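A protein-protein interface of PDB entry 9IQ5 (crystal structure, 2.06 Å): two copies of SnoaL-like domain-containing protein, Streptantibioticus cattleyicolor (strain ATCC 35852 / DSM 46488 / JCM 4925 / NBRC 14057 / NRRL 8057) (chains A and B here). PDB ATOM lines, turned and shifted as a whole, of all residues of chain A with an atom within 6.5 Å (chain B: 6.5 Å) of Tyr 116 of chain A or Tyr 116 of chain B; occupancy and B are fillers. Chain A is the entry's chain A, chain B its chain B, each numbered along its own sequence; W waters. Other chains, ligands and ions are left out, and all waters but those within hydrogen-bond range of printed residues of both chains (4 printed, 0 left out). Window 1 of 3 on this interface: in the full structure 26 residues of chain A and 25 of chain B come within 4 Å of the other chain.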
ATOM      1  N   ILE A  32      -3.344 -12.201  -1.685  1.00  0.00           N
ATOM      2  CA  ILE A  32      -1.944 -12.543  -1.955  1.00  0.00           C
ATOM      3  C   ILE A  32      -1.701 -12.437  -3.462  1.00  0.00           C
ATOM      4  O   ILE A  32      -2.289 -13.193  -4.248  1.00  0.00           O
ATOM      5  CB  ILE A  32      -1.588 -13.945  -1.424  1.00  0.00           C
ATOM      6  CG1 ILE A  32      -2.003 -14.070   0.047  1.00  0.00           C
ATOM      7  CG2 ILE A  32      -0.074 -14.194  -1.593  1.00  0.00           C
ATOM      8  CD1 ILE A  32      -1.454 -15.303   0.773  1.00  0.00           C
ATOM      9  N   THR A  33      -0.822 -11.512  -3.850  1.00  0.00           N
ATOM     10  CA  THR A  33      -0.542 -11.172  -5.245  1.00  0.00           C
ATOM     11  C   THR A  33       0.224 -12.311  -5.918  1.00  0.00           C
ATOM     12  O   THR A  33       0.730 -13.210  -5.242  1.00  0.00           O
ATOM     13  CB  THR A  33       0.292  -9.889  -5.309  1.00  0.00           C
ATOM     14  OG1 THR A  33       1.594 -10.215  -4.852  1.00  0.00           O
ATOM     15  CG2 THR A  33      -0.249  -8.783  -4.405  1.00  0.00           C
ATOM     16  N   PRO A  34       0.355 -12.283  -7.254  1.00  0.00           N
ATOM     17  CA  PRO A  34       1.023 -13.392  -7.954  1.00  0.00           C
ATOM     18  C   PRO A  34       2.538 -13.340  -7.955  1.00  0.00           C
ATOM     19  O   PRO A  34       3.167 -14.326  -8.381  1.00  0.00           O
ATOM     20  CB  PRO A  34       0.499 -13.255  -9.393  1.00  0.00           C
ATOM     21  CG  PRO A  34       0.204 -11.809  -9.544  1.00  0.00           C
ATOM     22  CD  PRO A  34      -0.295 -11.359  -8.197  1.00  0.00           C
ATOM     23  N   ARG A  85     -10.940 -17.651 -13.464  1.00  0.00           N
ATOM     24  CA  ARG A  85      -9.926 -17.639 -14.503  1.00  0.00           C
ATOM     25  C   ARG A  85      -9.853 -16.255 -15.129  1.00  0.00           C
ATOM     26  O   ARG A  85     -10.886 -15.606 -15.366  1.00  0.00           O
ATOM     27  CB  ARG A  85     -10.241 -18.691 -15.573  1.00  0.00           C
ATOM     28  CG  ARG A  85     -10.522 -20.114 -14.999  1.00  0.00           C
ATOM     29  CD  ARG A  85     -10.483 -21.207 -16.073  1.00  0.00           C
ATOM     30  NE  ARG A  85      -9.078 -21.428 -16.389  1.00  0.00           N
ATOM     31  CZ  ARG A  85      -8.310 -22.397 -15.898  1.00  0.00           C
ATOM     32  NH1 ARG A  85      -8.820 -23.399 -15.192  1.00  0.00           N
ATOM     33  NH2 ARG A  85      -6.984 -22.315 -16.059  1.00  0.00           N
ATOM     34  N   TRP A  86      -8.634 -15.796 -15.417  1.00  0.00           N
ATOM     35  CA  TRP A  86      -8.504 -14.496 -16.060  1.00  0.00           C
ATOM     36  C   TRP A  86      -7.451 -14.554 -17.155  1.00  0.00           C
ATOM     37  O   TRP A  86      -6.626 -15.476 -17.225  1.00  0.00           O
ATOM     38  CB  TRP A  86      -8.183 -13.378 -15.062  1.00  0.00           C
ATOM     39  CG  TRP A  86      -6.972 -13.610 -14.175  1.00  0.00           C
ATOM     40  CD1 TRP A  86      -6.975 -14.109 -12.897  1.00  0.00           C
ATOM     41  CD2 TRP A  86      -5.590 -13.338 -14.498  1.00  0.00           C
ATOM     42  NE1 TRP A  86      -5.685 -14.142 -12.405  1.00  0.00           N
ATOM     43  CE2 TRP A  86      -4.819 -13.685 -13.365  1.00  0.00           C
ATOM     44  CE3 TRP A  86      -4.935 -12.828 -15.636  1.00  0.00           C
ATOM     45  CZ2 TRP A  86      -3.430 -13.539 -13.329  1.00  0.00           C
ATOM     46  CZ3 TRP A  86      -3.567 -12.673 -15.609  1.00  0.00           C
ATOM     47  CH2 TRP A  86      -2.814 -13.045 -14.458  1.00  0.00           C
ATOM     48  N   ARG A  98      -2.272 -15.616 -18.946  1.00  0.00           N
ATOM     49  CA  ARG A  98      -3.370 -16.331 -18.303  1.00  0.00           C
ATOM     50  C   ARG A  98      -3.025 -16.548 -16.840  1.00  0.00           C
ATOM     51  O   ARG A  98      -1.858 -16.769 -16.502  1.00  0.00           O
ATOM     52  CB  ARG A  98      -3.636 -17.732 -18.915  1.00  0.00           C
ATOM     53  CG  ARG A  98      -4.192 -17.770 -20.296  1.00  0.00           C
ATOM     54  CD  ARG A  98      -4.465 -19.231 -20.723  1.00  0.00           C
ATOM     55  NE  ARG A  98      -4.894 -19.287 -22.118  1.00  0.00           N
ATOM     56  CZ  ARG A  98      -6.101 -18.912 -22.533  1.00  0.00           C
ATOM     57  NH1 ARG A  98      -7.028 -18.484 -21.680  1.00  0.00           N
ATOM     58  NH2 ARG A  98      -6.391 -18.965 -23.835  1.00  0.00           N
ATOM     59  N   GLY A  99      -4.057 -16.580 -16.000  1.00  0.00           N
ATOM     60  CA  GLY A  99      -3.904 -16.903 -14.599  1.00  0.00           C
ATOM     61  C   GLY A  99      -5.217 -17.302 -13.944  1.00  0.00           C
ATOM     62  O   GLY A  99      -6.227 -17.558 -14.614  1.00  0.00           O
ATOM     63  N   VAL A 100      -5.181 -17.386 -12.609  1.00  0.00           N
ATOM     64  CA  VAL A 100      -6.357 -17.729 -11.820  1.00  0.00           C
ATOM     65  C   VAL A 100      -6.326 -16.900 -10.550  1.00  0.00           C
ATOM     66  O   VAL A 100      -5.255 -16.515 -10.074  1.00  0.00           O
ATOM     67  CB  VAL A 100      -6.465 -19.241 -11.447  1.00  0.00           C
ATOM     68  CG1 VAL A 100      -6.633 -20.080 -12.658  1.00  0.00           C
ATOM     69  CG2 VAL A 100      -5.245 -19.709 -10.632  1.00  0.00           C
ATOM     70  N   ASP A 101      -7.519 -16.575 -10.040  1.00  0.00           N
ATOM     71  CA  ASP A 101      -7.713 -16.122  -8.670  1.00  0.00           C
ATOM     72  C   ASP A 101      -8.410 -17.252  -7.954  1.00  0.00           C
ATOM     73  O   ASP A 101      -9.408 -17.780  -8.457  1.00  0.00           O
ATOM     74  CB  ASP A 101      -8.590 -14.870  -8.546  1.00  0.00           C
ATOM     75  CG  ASP A 101      -7.983 -13.605  -9.123  1.00  0.00           C
ATOM     76  OD1 ASP A 101      -6.770 -13.566  -9.501  1.00  0.00           O
ATOM     77  OD2 ASP A 101      -8.784 -12.611  -9.191  1.00  0.00           O
ATOM     78  N   LEU A 102      -7.865 -17.641  -6.807  1.00  0.00           N
ATOM     79  CA  LEU A 102      -8.461 -18.622  -5.924  1.00  0.00           C
ATOM     80  C   LEU A 102      -9.127 -17.886  -4.783  1.00  0.00           C
ATOM     81  O   LEU A 102      -8.457 -17.150  -4.052  1.00  0.00           O
ATOM     82  CB  LEU A 102      -7.387 -19.557  -5.369  1.00  0.00           C
ATOM     83  CG  LEU A 102      -7.245 -20.870  -6.109  1.00  0.00           C
ATOM     84  CD1 LEU A 102      -7.286 -20.692  -7.609  1.00  0.00           C
ATOM     85  CD2 LEU A 102      -5.967 -21.547  -5.657  1.00  0.00           C
ATOM     86  N   ASP A 114      -6.164 -15.613  -3.585  1.00  0.00           N
ATOM     87  CA  ASP A 114      -4.774 -16.041  -3.829  1.00  0.00           C
ATOM     88  C   ASP A 114      -4.585 -16.057  -5.337  1.00  0.00           C
ATOM     89  O   ASP A 114      -5.252 -16.829  -6.041  1.00  0.00           O
ATOM     90  CB  ASP A 114      -4.521 -17.427  -3.195  1.00  0.00           C
ATOM     91  CG  ASP A 114      -3.020 -17.792  -3.047  1.00  0.00           C
ATOM     92  OD1 ASP A 114      -2.139 -16.934  -3.261  1.00  0.00           O
ATOM     93  OD2 ASP A 114      -2.725 -18.976  -2.695  1.00  0.00           O
ATOM     94  N   VAL A 115      -3.733 -15.177  -5.846  1.00  0.00           N
ATOM     95  CA  VAL A 115      -3.652 -14.881  -7.277  1.00  0.00           C
ATOM     96  C   VAL A 115      -2.431 -15.573  -7.865  1.00  0.00           C
ATOM     97  O   VAL A 115      -1.353 -15.556  -7.265  1.00  0.00           O
ATOM     98  CB  VAL A 115      -3.590 -13.352  -7.507  1.00  0.00           C
ATOM     99  CG1 VAL A 115      -3.656 -12.996  -8.993  1.00  0.00           C
ATOM    100  CG2 VAL A 115      -4.729 -12.673  -6.780  1.00  0.00           C
ATOM    101  N   TYR A 116      -2.594 -16.179  -9.042  1.00  0.00           N
ATOM    102  CA  TYR A 116      -1.488 -16.810  -9.753  1.00  0.00           C
ATOM    103  C   TYR A 116      -1.550 -16.442 -11.229  1.00  0.00           C
ATOM    104  O   TYR A 116      -2.631 -16.249 -11.797  1.00  0.00           O
ATOM    105  CB  TYR A 116      -1.491 -18.340  -9.606  1.00  0.00           C
ATOM    106  CG  TYR A 116      -1.280 -18.783  -8.166  1.00  0.00           C
ATOM    107  CD1 TYR A 116       0.007 -18.890  -7.607  1.00  0.00           C
ATOM    108  CD2 TYR A 116      -2.362 -19.022  -7.362  1.00  0.00           C
ATOM    109  CE1 TYR A 116       0.174 -19.281  -6.267  1.00  0.00           C
ATOM    110  CE2 TYR A 116      -2.215 -19.379  -6.058  1.00  0.00           C
ATOM    111  CZ  TYR A 116      -0.952 -19.514  -5.504  1.00  0.00           C
ATOM    112  OH  TYR A 116      -0.894 -19.880  -4.184  1.00  0.00           O
ATOM    113  N   ARG A 117      -0.377 -16.299 -11.836  1.00  0.00           N
ATOM    114  CA  ARG A 117      -0.263 -16.105 -13.272  1.00  0.00           C
ATOM    115  C   ARG A 117       0.700 -17.143 -13.830  1.00  0.00           C
ATOM    116  O   ARG A 117       1.637 -17.547 -13.140  1.00  0.00           O
ATOM    117  CB  ARG A 117       0.222 -14.690 -13.594  1.00  0.00           C
ATOM    118  CG  ARG A 117       1.639 -14.406 -13.099  1.00  0.00           C
ATOM    119  CD  ARG A 117       2.286 -13.214 -13.845  1.00  0.00           C
ATOM    120  NE  ARG A 117       1.907 -11.923 -13.284  1.00  0.00           N
ATOM    121  CZ  ARG A 117       1.113 -11.044 -13.882  1.00  0.00           C
ATOM    122  NH1 ARG A 117       0.548 -11.304 -15.054  1.00  0.00           N
ATOM    123  NH2 ARG A 117       0.890  -9.870 -13.298  1.00  0.00           N
ATOM    124  N   LYS A 118       0.422 -17.640 -15.037  1.00  0.00           N
ATOM    125  CA  LYS A 118       1.436 -18.380 -15.777  1.00  0.00           C
ATOM    126  C   LYS A 118       2.617 -17.456 -16.034  1.00  0.00           C
ATOM    127  O   LYS A 118       2.447 -16.244 -16.154  1.00  0.00           O
ATOM    128  CB  LYS A 118       0.873 -18.917 -17.097  1.00  0.00           C
ATOM    129  CG  LYS A 118      -0.259 -19.916 -16.934  1.00  0.00           C
ATOM    130  CD  LYS A 118       0.178 -21.167 -16.178  1.00  0.00           C
ATOM    131  CE  LYS A 118      -0.904 -22.251 -16.253  1.00  0.00           C
ATOM    132  NZ  LYS A 118      -0.483 -23.503 -15.525  1.00  0.00           N
ATOM    133  N   ILE B  32      -0.733 -29.081 -17.163  1.00  0.00           N
ATOM    134  CA  ILE B  32      -0.352 -27.772 -17.674  1.00  0.00           C
ATOM    135  C   ILE B  32       0.680 -27.190 -16.726  1.00  0.00           C
ATOM    136  O   ILE B  32       0.408 -27.043 -15.528  1.00  0.00           O
ATOM    137  CB  ILE B  32      -1.565 -26.838 -17.829  1.00  0.00           C
ATOM    138  CG1 ILE B  32      -2.660 -27.535 -18.649  1.00  0.00           C
ATOM    139  CG2 ILE B  32      -1.133 -25.558 -18.472  1.00  0.00           C
ATOM    140  CD1 ILE B  32      -3.825 -26.618 -19.076  1.00  0.00           C
ATOM    141  N   THR B  33       1.884 -26.919 -17.252  1.00  0.00           N
ATOM    142  CA  THR B  33       3.005 -26.411 -16.466  1.00  0.00           C
ATOM    143  C   THR B  33       2.765 -24.955 -16.067  1.00  0.00           C
ATOM    144  O   THR B  33       1.883 -24.280 -16.608  1.00  0.00           O
ATOM    145  CB  THR B  33       4.315 -26.509 -17.260  1.00  0.00           C
ATOM    146  OG1 THR B  33       4.312 -25.508 -18.296  1.00  0.00           O
ATOM    147  CG2 THR B  33       4.498 -27.891 -17.873  1.00  0.00           C
ATOM    148  N   PRO B  34       3.550 -24.431 -15.120  1.00  0.00           N
ATOM    149  CA  PRO B  34       3.344 -23.046 -14.676  1.00  0.00           C
ATOM    150  C   PRO B  34       4.002 -22.003 -15.559  1.00  0.00           C
ATOM    151  O   PRO B  34       3.842 -20.805 -15.288  1.00  0.00           O
ATOM    152  CB  PRO B  34       3.977 -23.038 -13.284  1.00  0.00           C
ATOM    153  CG  PRO B  34       5.003 -24.046 -13.369  1.00  0.00           C
ATOM    154  CD  PRO B  34       4.495 -25.128 -14.239  1.00  0.00           C
ATOM    155  N   ARG B  85      -0.855 -27.435  -2.085  1.00  0.00           N
ATOM    156  CA  ARG B  85       0.137 -26.370  -1.938  1.00  0.00           C
ATOM    157  C   ARG B  85       1.543 -26.957  -1.869  1.00  0.00           C
ATOM    158  O   ARG B  85       1.763 -28.045  -1.312  1.00  0.00           O
ATOM    159  CB  ARG B  85      -0.154 -25.520  -0.697  1.00  0.00           C
ATOM    160  CG  ARG B  85      -1.613 -25.010  -0.675  1.00  0.00           C
ATOM    161  CD  ARG B  85      -1.937 -23.988   0.411  1.00  0.00           C
ATOM    162  NE  ARG B  85      -1.414 -22.658   0.150  1.00  0.00           N
ATOM    163  CZ  ARG B  85      -2.100 -21.673  -0.426  1.00  0.00           C
ATOM    164  NH1 ARG B  85      -3.384 -21.803  -0.734  1.00  0.00           N
ATOM    165  NH2 ARG B  85      -1.488 -20.515  -0.672  1.00  0.00           N
ATOM    166  N   TRP B  86       2.499 -26.260  -2.468  1.00  0.00           N
ATOM    167  CA  TRP B  86       3.869 -26.739  -2.422  1.00  0.00           C
ATOM    168  C   TRP B  86       4.813 -25.567  -2.245  1.00  0.00           C
ATOM    169  O   TRP B  86       4.452 -24.400  -2.433  1.00  0.00           O
ATOM    170  CB  TRP B  86       4.234 -27.551  -3.671  1.00  0.00           C
ATOM    171  CG  TRP B  86       3.959 -26.845  -4.980  1.00  0.00           C
ATOM    172  CD1 TRP B  86       2.845 -26.976  -5.766  1.00  0.00           C
ATOM    173  CD2 TRP B  86       4.818 -25.928  -5.655  1.00  0.00           C
ATOM    174  NE1 TRP B  86       2.958 -26.180  -6.889  1.00  0.00           N
ATOM    175  CE2 TRP B  86       4.160 -25.528  -6.843  1.00  0.00           C
ATOM    176  CE3 TRP B  86       6.082 -25.401  -5.373  1.00  0.00           C
ATOM    177  CZ2 TRP B  86       4.726 -24.638  -7.739  1.00  0.00           C
ATOM    178  CZ3 TRP B  86       6.639 -24.514  -6.266  1.00  0.00           C
ATOM    179  CH2 TRP B  86       5.963 -24.131  -7.428  1.00  0.00           C
ATOM    180  N   ARG B  98       6.937 -20.689  -3.738  1.00  0.00           N
ATOM    181  CA  ARG B  98       5.643 -21.279  -3.370  1.00  0.00           C
ATOM    182  C   ARG B  98       4.753 -21.409  -4.597  1.00  0.00           C
ATOM    183  O   ARG B  98       4.830 -20.598  -5.524  1.00  0.00           O
ATOM    184  CB  ARG B  98       4.817 -20.410  -2.390  1.00  0.00           C
ATOM    185  CG  ARG B  98       5.396 -20.221  -1.023  1.00  0.00           C
ATOM    186  CD  ARG B  98       4.442 -19.408  -0.128  1.00  0.00           C
ATOM    187  NE  ARG B  98       5.132 -19.002   1.096  1.00  0.00           N
ATOM    188  CZ  ARG B  98       5.415 -19.799   2.122  1.00  0.00           C
ATOM    189  NH1 ARG B  98       5.035 -21.071   2.145  1.00  0.00           N
ATOM    190  NH2 ARG B  98       6.084 -19.303   3.161  1.00  0.00           N
ATOM    191  N   GLY B  99       3.866 -22.391  -4.569  1.00  0.00           N
ATOM    192  CA  GLY B  99       2.864 -22.511  -5.601  1.00  0.00           C
ATOM    193  C   GLY B  99       1.741 -23.454  -5.213  1.00  0.00           C
ATOM    194  O   GLY B  99       1.609 -23.872  -4.056  1.00  0.00           O
ATOM    195  N   VAL B 100       0.931 -23.797  -6.213  1.00  0.00           N
ATOM    196  CA  VAL B 100      -0.164 -24.731  -6.031  1.00  0.00           C
ATOM    197  C   VAL B 100      -0.246 -25.606  -7.260  1.00  0.00           C
ATOM    198  O   VAL B 100       0.136 -25.198  -8.357  1.00  0.00           O
ATOM    199  CB  VAL B 100      -1.543 -24.060  -5.819  1.00  0.00           C
ATOM    200  CG1 VAL B 100      -1.578 -23.248  -4.566  1.00  0.00           C
ATOM    201  CG2 VAL B 100      -1.936 -23.255  -7.036  1.00  0.00           C
ATOM    202  N   ASP B 101      -0.727 -26.827  -7.053  1.00  0.00           N
ATOM    203  CA  ASP B 101      -1.241 -27.674  -8.107  1.00  0.00           C
ATOM    204  C   ASP B 101      -2.755 -27.713  -7.940  1.00  0.00           C
ATOM    205  O   ASP B 101      -3.254 -28.033  -6.853  1.00  0.00           O
ATOM    206  CB  ASP B 101      -0.715 -29.113  -8.009  1.00  0.00           C
ATOM    207  CG  ASP B 101       0.810 -29.237  -8.125  1.00  0.00           C
ATOM    208  OD1 ASP B 101       1.512 -28.237  -8.406  1.00  0.00           O
ATOM    209  OD2 ASP B 101       1.303 -30.382  -7.920  1.00  0.00           O
ATOM    210  N   LEU B 102      -3.476 -27.442  -9.016  1.00  0.00           N
ATOM    211  CA  LEU B 102      -4.923 -27.582  -9.061  1.00  0.00           C
ATOM    212  C   LEU B 102      -5.245 -28.879  -9.780  1.00  0.00           C
ATOM    213  O   LEU B 102      -4.864 -29.045 -10.941  1.00  0.00           O
ATOM    214  CB  LEU B 102      -5.540 -26.411  -9.818  1.00  0.00           C
ATOM    215  CG  LEU B 102      -6.022 -25.234  -8.988  1.00  0.00           C
ATOM    216  CD1 LEU B 102      -5.061 -24.923  -7.884  1.00  0.00           C
ATOM    217  CD2 LEU B 102      -6.164 -24.021  -9.894  1.00  0.00           C
ATOM    218  N   ASP B 114      -3.089 -28.507 -13.020  1.00  0.00           N
ATOM    219  CA  ASP B 114      -2.810 -27.147 -13.472  1.00  0.00           C
ATOM    220  C   ASP B 114      -1.870 -26.531 -12.447  1.00  0.00           C
ATOM    221  O   ASP B 114      -2.267 -26.313 -11.294  1.00  0.00           O
ATOM    222  CB  ASP B 114      -4.110 -26.326 -13.590  1.00  0.00           C
ATOM    223  CG  ASP B 114      -3.967 -25.087 -14.501  1.00  0.00           C
ATOM    224  OD1 ASP B 114      -2.960 -24.998 -15.231  1.00  0.00           O
ATOM    225  OD2 ASP B 114      -4.833 -24.169 -14.455  1.00  0.00           O
ATOM    226  N   VAL B 115      -0.630 -26.239 -12.852  1.00  0.00           N
ATOM    227  CA  VAL B 115       0.408 -25.865 -11.903  1.00  0.00           C
ATOM    228  C   VAL B 115       0.637 -24.363 -11.964  1.00  0.00           C
ATOM    229  O   VAL B 115       0.728 -23.771 -13.050  1.00  0.00           O
ATOM    230  CB  VAL B 115       1.722 -26.628 -12.158  1.00  0.00           C
ATOM    231  CG1 VAL B 115       2.668 -26.362 -11.037  1.00  0.00           C
ATOM    232  CG2 VAL B 115       1.483 -28.134 -12.268  1.00  0.00           C
ATOM    233  N   TYR B 116       0.771 -23.746 -10.794  1.00  0.00           N
ATOM    234  CA  TYR B 116       1.081 -22.334 -10.709  1.00  0.00           C
ATOM    235  C   TYR B 116       2.145 -22.094  -9.652  1.00  0.00           C
ATOM    236  O   TYR B 116       2.137 -22.734  -8.601  1.00  0.00           O
ATOM    237  CB  TYR B 116      -0.166 -21.517 -10.368  1.00  0.00           C
ATOM    238  CG  TYR B 116      -1.232 -21.589 -11.426  1.00  0.00           C
ATOM    239  CD1 TYR B 116      -2.118 -22.654 -11.462  1.00  0.00           C
ATOM    240  CD2 TYR B 116      -1.349 -20.595 -12.401  1.00  0.00           C
ATOM    241  CE1 TYR B 116      -3.078 -22.746 -12.434  1.00  0.00           C
ATOM    242  CE2 TYR B 116      -2.325 -20.681 -13.389  1.00  0.00           C
ATOM    243  CZ  TYR B 116      -3.179 -21.750 -13.398  1.00  0.00           C
ATOM    244  OH  TYR B 116      -4.155 -21.858 -14.364  1.00  0.00           O
ATOM    245  N   ARG B 117       3.041 -21.150  -9.925  1.00  0.00           N
ATOM    246  CA  ARG B 117       4.034 -20.714  -8.952  1.00  0.00           C
ATOM    247  C   ARG B 117       3.958 -19.202  -8.789  1.00  0.00           C
ATOM    248  O   ARG B 117       3.604 -18.490  -9.736  1.00  0.00           O
ATOM    249  CB  ARG B 117       5.438 -21.083  -9.378  1.00  0.00           C
ATOM    250  CG  ARG B 117       5.866 -20.336 -10.599  1.00  0.00           C
ATOM    251  CD  ARG B 117       7.379 -20.306 -10.746  1.00  0.00           C
ATOM    252  NE  ARG B 117       7.908 -21.492 -11.401  1.00  0.00           N
ATOM    253  CZ  ARG B 117       8.656 -22.419 -10.809  1.00  0.00           C
ATOM    254  NH1 ARG B 117       8.958 -22.355  -9.519  1.00  0.00           N
ATOM    255  NH2 ARG B 117       9.127 -23.430 -11.534  1.00  0.00           N
ATOM    256  N   LYS B 118       4.229 -18.729  -7.575  1.00  0.00           N
ATOM    257  CA  LYS B 118       4.481 -17.314  -7.368  1.00  0.00           C
ATOM    258  C   LYS B 118       5.730 -16.891  -8.161  1.00  0.00           C
ATOM    259  O   LYS B 118       6.653 -17.673  -8.362  1.00  0.00           O
ATOM    260  CB  LYS B 118       4.629 -17.038  -5.872  1.00  0.00           C
ATOM    261  CG  LYS B 118       3.363 -17.384  -5.030  1.00  0.00           C
ATOM    262  CD  LYS B 118       2.131 -16.536  -5.422  1.00  0.00           C
ATOM    263  CE  LYS B 118       0.946 -16.659  -4.420  1.00  0.00           C
ATOM    264  NZ  LYS B 118      -0.228 -15.816  -4.865  1.00  0.00           N
HETATM  265  O   HOH W   1       2.592 -20.140 -12.700  1.00  0.00           O
HETATM  266  O   HOH W   2      -4.163 -20.425 -16.576  1.00  0.00           O
HETATM  267  O   HOH W   3       0.036 -18.070  -1.329  1.00  0.00           O
HETATM  268  O   HOH W   4       1.884 -16.252  -9.682  1.00  0.00           O
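The guanidinium group (NH2) of Arg 85 of chain A lies within hydrogen-bond range of the side-chain hydroxyl (OH) of Tyr 116 of chain B (3.3 Å). The side-chain amino group (NZ) of Lys 118 of chain A is in hydrogen-bond range of the backbone carbonyl oxygen (O) of Thr 33 of chain B (2.7 Å). The side-chain carboxylate (OD2) of Asp 114 of chain A is in salt-bridge range of the guanidinium group (NH2) of Arg 85 of chain B, 2.8 Å away. The backbone carbonyl oxygen (O) of Thr 33 of chain A is in hydrogen-bond range of the side-chain amino group (NZ) of Lys 118 of chain B (2.8 Å). O of Ile 32 of chain A is in hydrogen-bond range of NZ of Lys 118 of chain B (3.4 Å). The side-chain amino group (NZ) of Lys 118 of chain B lies within salt-bridge range of the side-chain carboxylate (OD1) of Asp 114 of chain A (2.7 Å). The side-chain amino group (NZ) of Lys 118 of chain A sits at hydrogen-bond distance from the backbone carbonyl oxygen (O) of Val 115 of chain B. The backbone carbonyl oxygen (O) of Val 115 of chain A sits at hydrogen-bond distance from the side-chain amino group (NZ) of Lys 118 of chain B (2.7 Å). The guanidinium group of Arg 85 of chain A is in salt-bridge range of the side-chain carboxylate of Asp 114 of chain B (3.3 Å). The side-chain amino group of Lys 118 of chain A lies within salt-bridge range of the side-chain carboxylate of Asp 114 of chain B (2.9 Å).
Water W2 lies within hydrogen-bond range of OH of Tyr 116 of chain B (2.6 Å) and NH2 of Arg 85 of chain A (3.4 Å). Water W4 lies within hydrogen-bond range of the backbone carbonyl oxygen of Pro 34 of chain A (2.7 Å), the backbone carbonyl oxygen of Arg 117 of chain B (2.8 Å) and the backbone NH of Arg 117 of chain A (3.1 Å). Water W1 lies within hydrogen-bond range of the backbone carbonyl oxygen of Arg 117 of chain A, the backbone carbonyl oxygen of Pro 34 of chain B and the backbone NH of Arg 117 of chain B. Water W3 bridges NH2 of Arg 85 of chain B and OD1 of Asp 114 of chain A.
Of the 15 printed residues of chain A, 9 touch a printed residue of chain B. Printed residues of chain A that touch a printed residue of chain B: Ile 32, Thr 33, Pro 34, Arg 85, Val 100, Asp 114, Val 115, Tyr 116 and Lys 118. Of the 15 printed residues of chain B, 9 touch a printed residue of chain A. Hydrophobic or aromatic side chains of chain B that line the printed part of chain A: Ile 32, Val 100 and Tyr 116. Among the printed residues, Asp or Glu carboxylates within 4 Å of a Lys or Arg side-chain nitrogen of the other chain: Arg 85 of chain A with Asp 114 of chain B (3.3 Å), Asp 114 of chain A with Arg 85 of chain B (2.8 Å), Asp 114 of chain A with Lys 118 of chain B (2.7 Å) and Lys 118 of chain A with Asp 114 of chain B (2.9 Å).
Among the printed residues, pairs that only touch across the chains: Tyr 116 of chain A with Lys 118 of chain B, Pro 34 of chain A with Lys 118 of chain B, Lys 118 of chain A with Pro 34 of chain B, Tyr 116 of chain A with Val 100 of chain B, Val 100 of chain A with Tyr 116 of chain B, Tyr 116 of chain A with Tyr 116 of chain B, Lys 118 of chain A with Tyr 116 of chain B, Tyr 116 of chain A with Arg 85 of chain B and Lys 118 of chain A with Ile 32 of chain B.
Tyr 116 of chain B touches just these residues of chain A: Arg 85 (3.3 Å), Val 100 (3.5 Å), Tyr 116 (3.5 Å) and Lys 118 (3.6 Å). Printed residues of chain A within 4 Å of Val 115 of chain B: Lys 118. Of the printed residues of chain A, Ile 32 of chain B touches Lys 118. Arg 98 of chain A touches none of the printed residues of chain B. The nearest printed residue of chain A that does not touch Tyr 116 of chain B is Arg 117 of chain A (4.3 Å). The nearest printed residue of chain B that does not touch Asp 114 of chain A is Val 100 of chain B (4.8 Å).
O of Ile 32 of chain A sits at hydrogen-bond distance from N of Val 115 of chain A (2.9 Å). O of Val 100 of chain A lies within hydrogen-bond range of NE1 of Trp 86 of chain A (3.4 Å). N of Asp 114 of chain A sits at hydrogen-bond distance from O of Leu 102 of chain A (2.8 Å). The backbone carbonyl oxygen (O) of Arg 98 of chain B lies within hydrogen-bond range of the backbone NH (N) of Lys 118 of chain B, at 2.8 Å. NE1 of Trp 86 of chain B sits close to O of Val 100 of chain B (3.3 Å). The side-chain hydroxyl of Tyr 116 of chain A sits at hydrogen-bond distance from the side-chain carboxylate of Asp 114 of chain A, 2.5 Å away.
Ile 32 of chain A touches Lys 118 of chain B, and with the chains exchanged Lys 118 of chain A touches Ile 32 of chain B. Pro 34 of chain A touches Lys 118 of chain B, and with the chains exchanged Lys 118 of chain A touches Pro 34 of chain B. Asp 114 of chain A touches Lys 118 of chain B, and with the chains exchanged Lys 118 of chain A touches Asp 114 of chain B. Tyr 116 of chain B touches its own counterpart, Tyr 116 of chain A. Positions printed for both chains: 32, 33, 34, 85, 86, 98, 99, 100, 101, 102, 114, 115, 116, 117 and 118.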
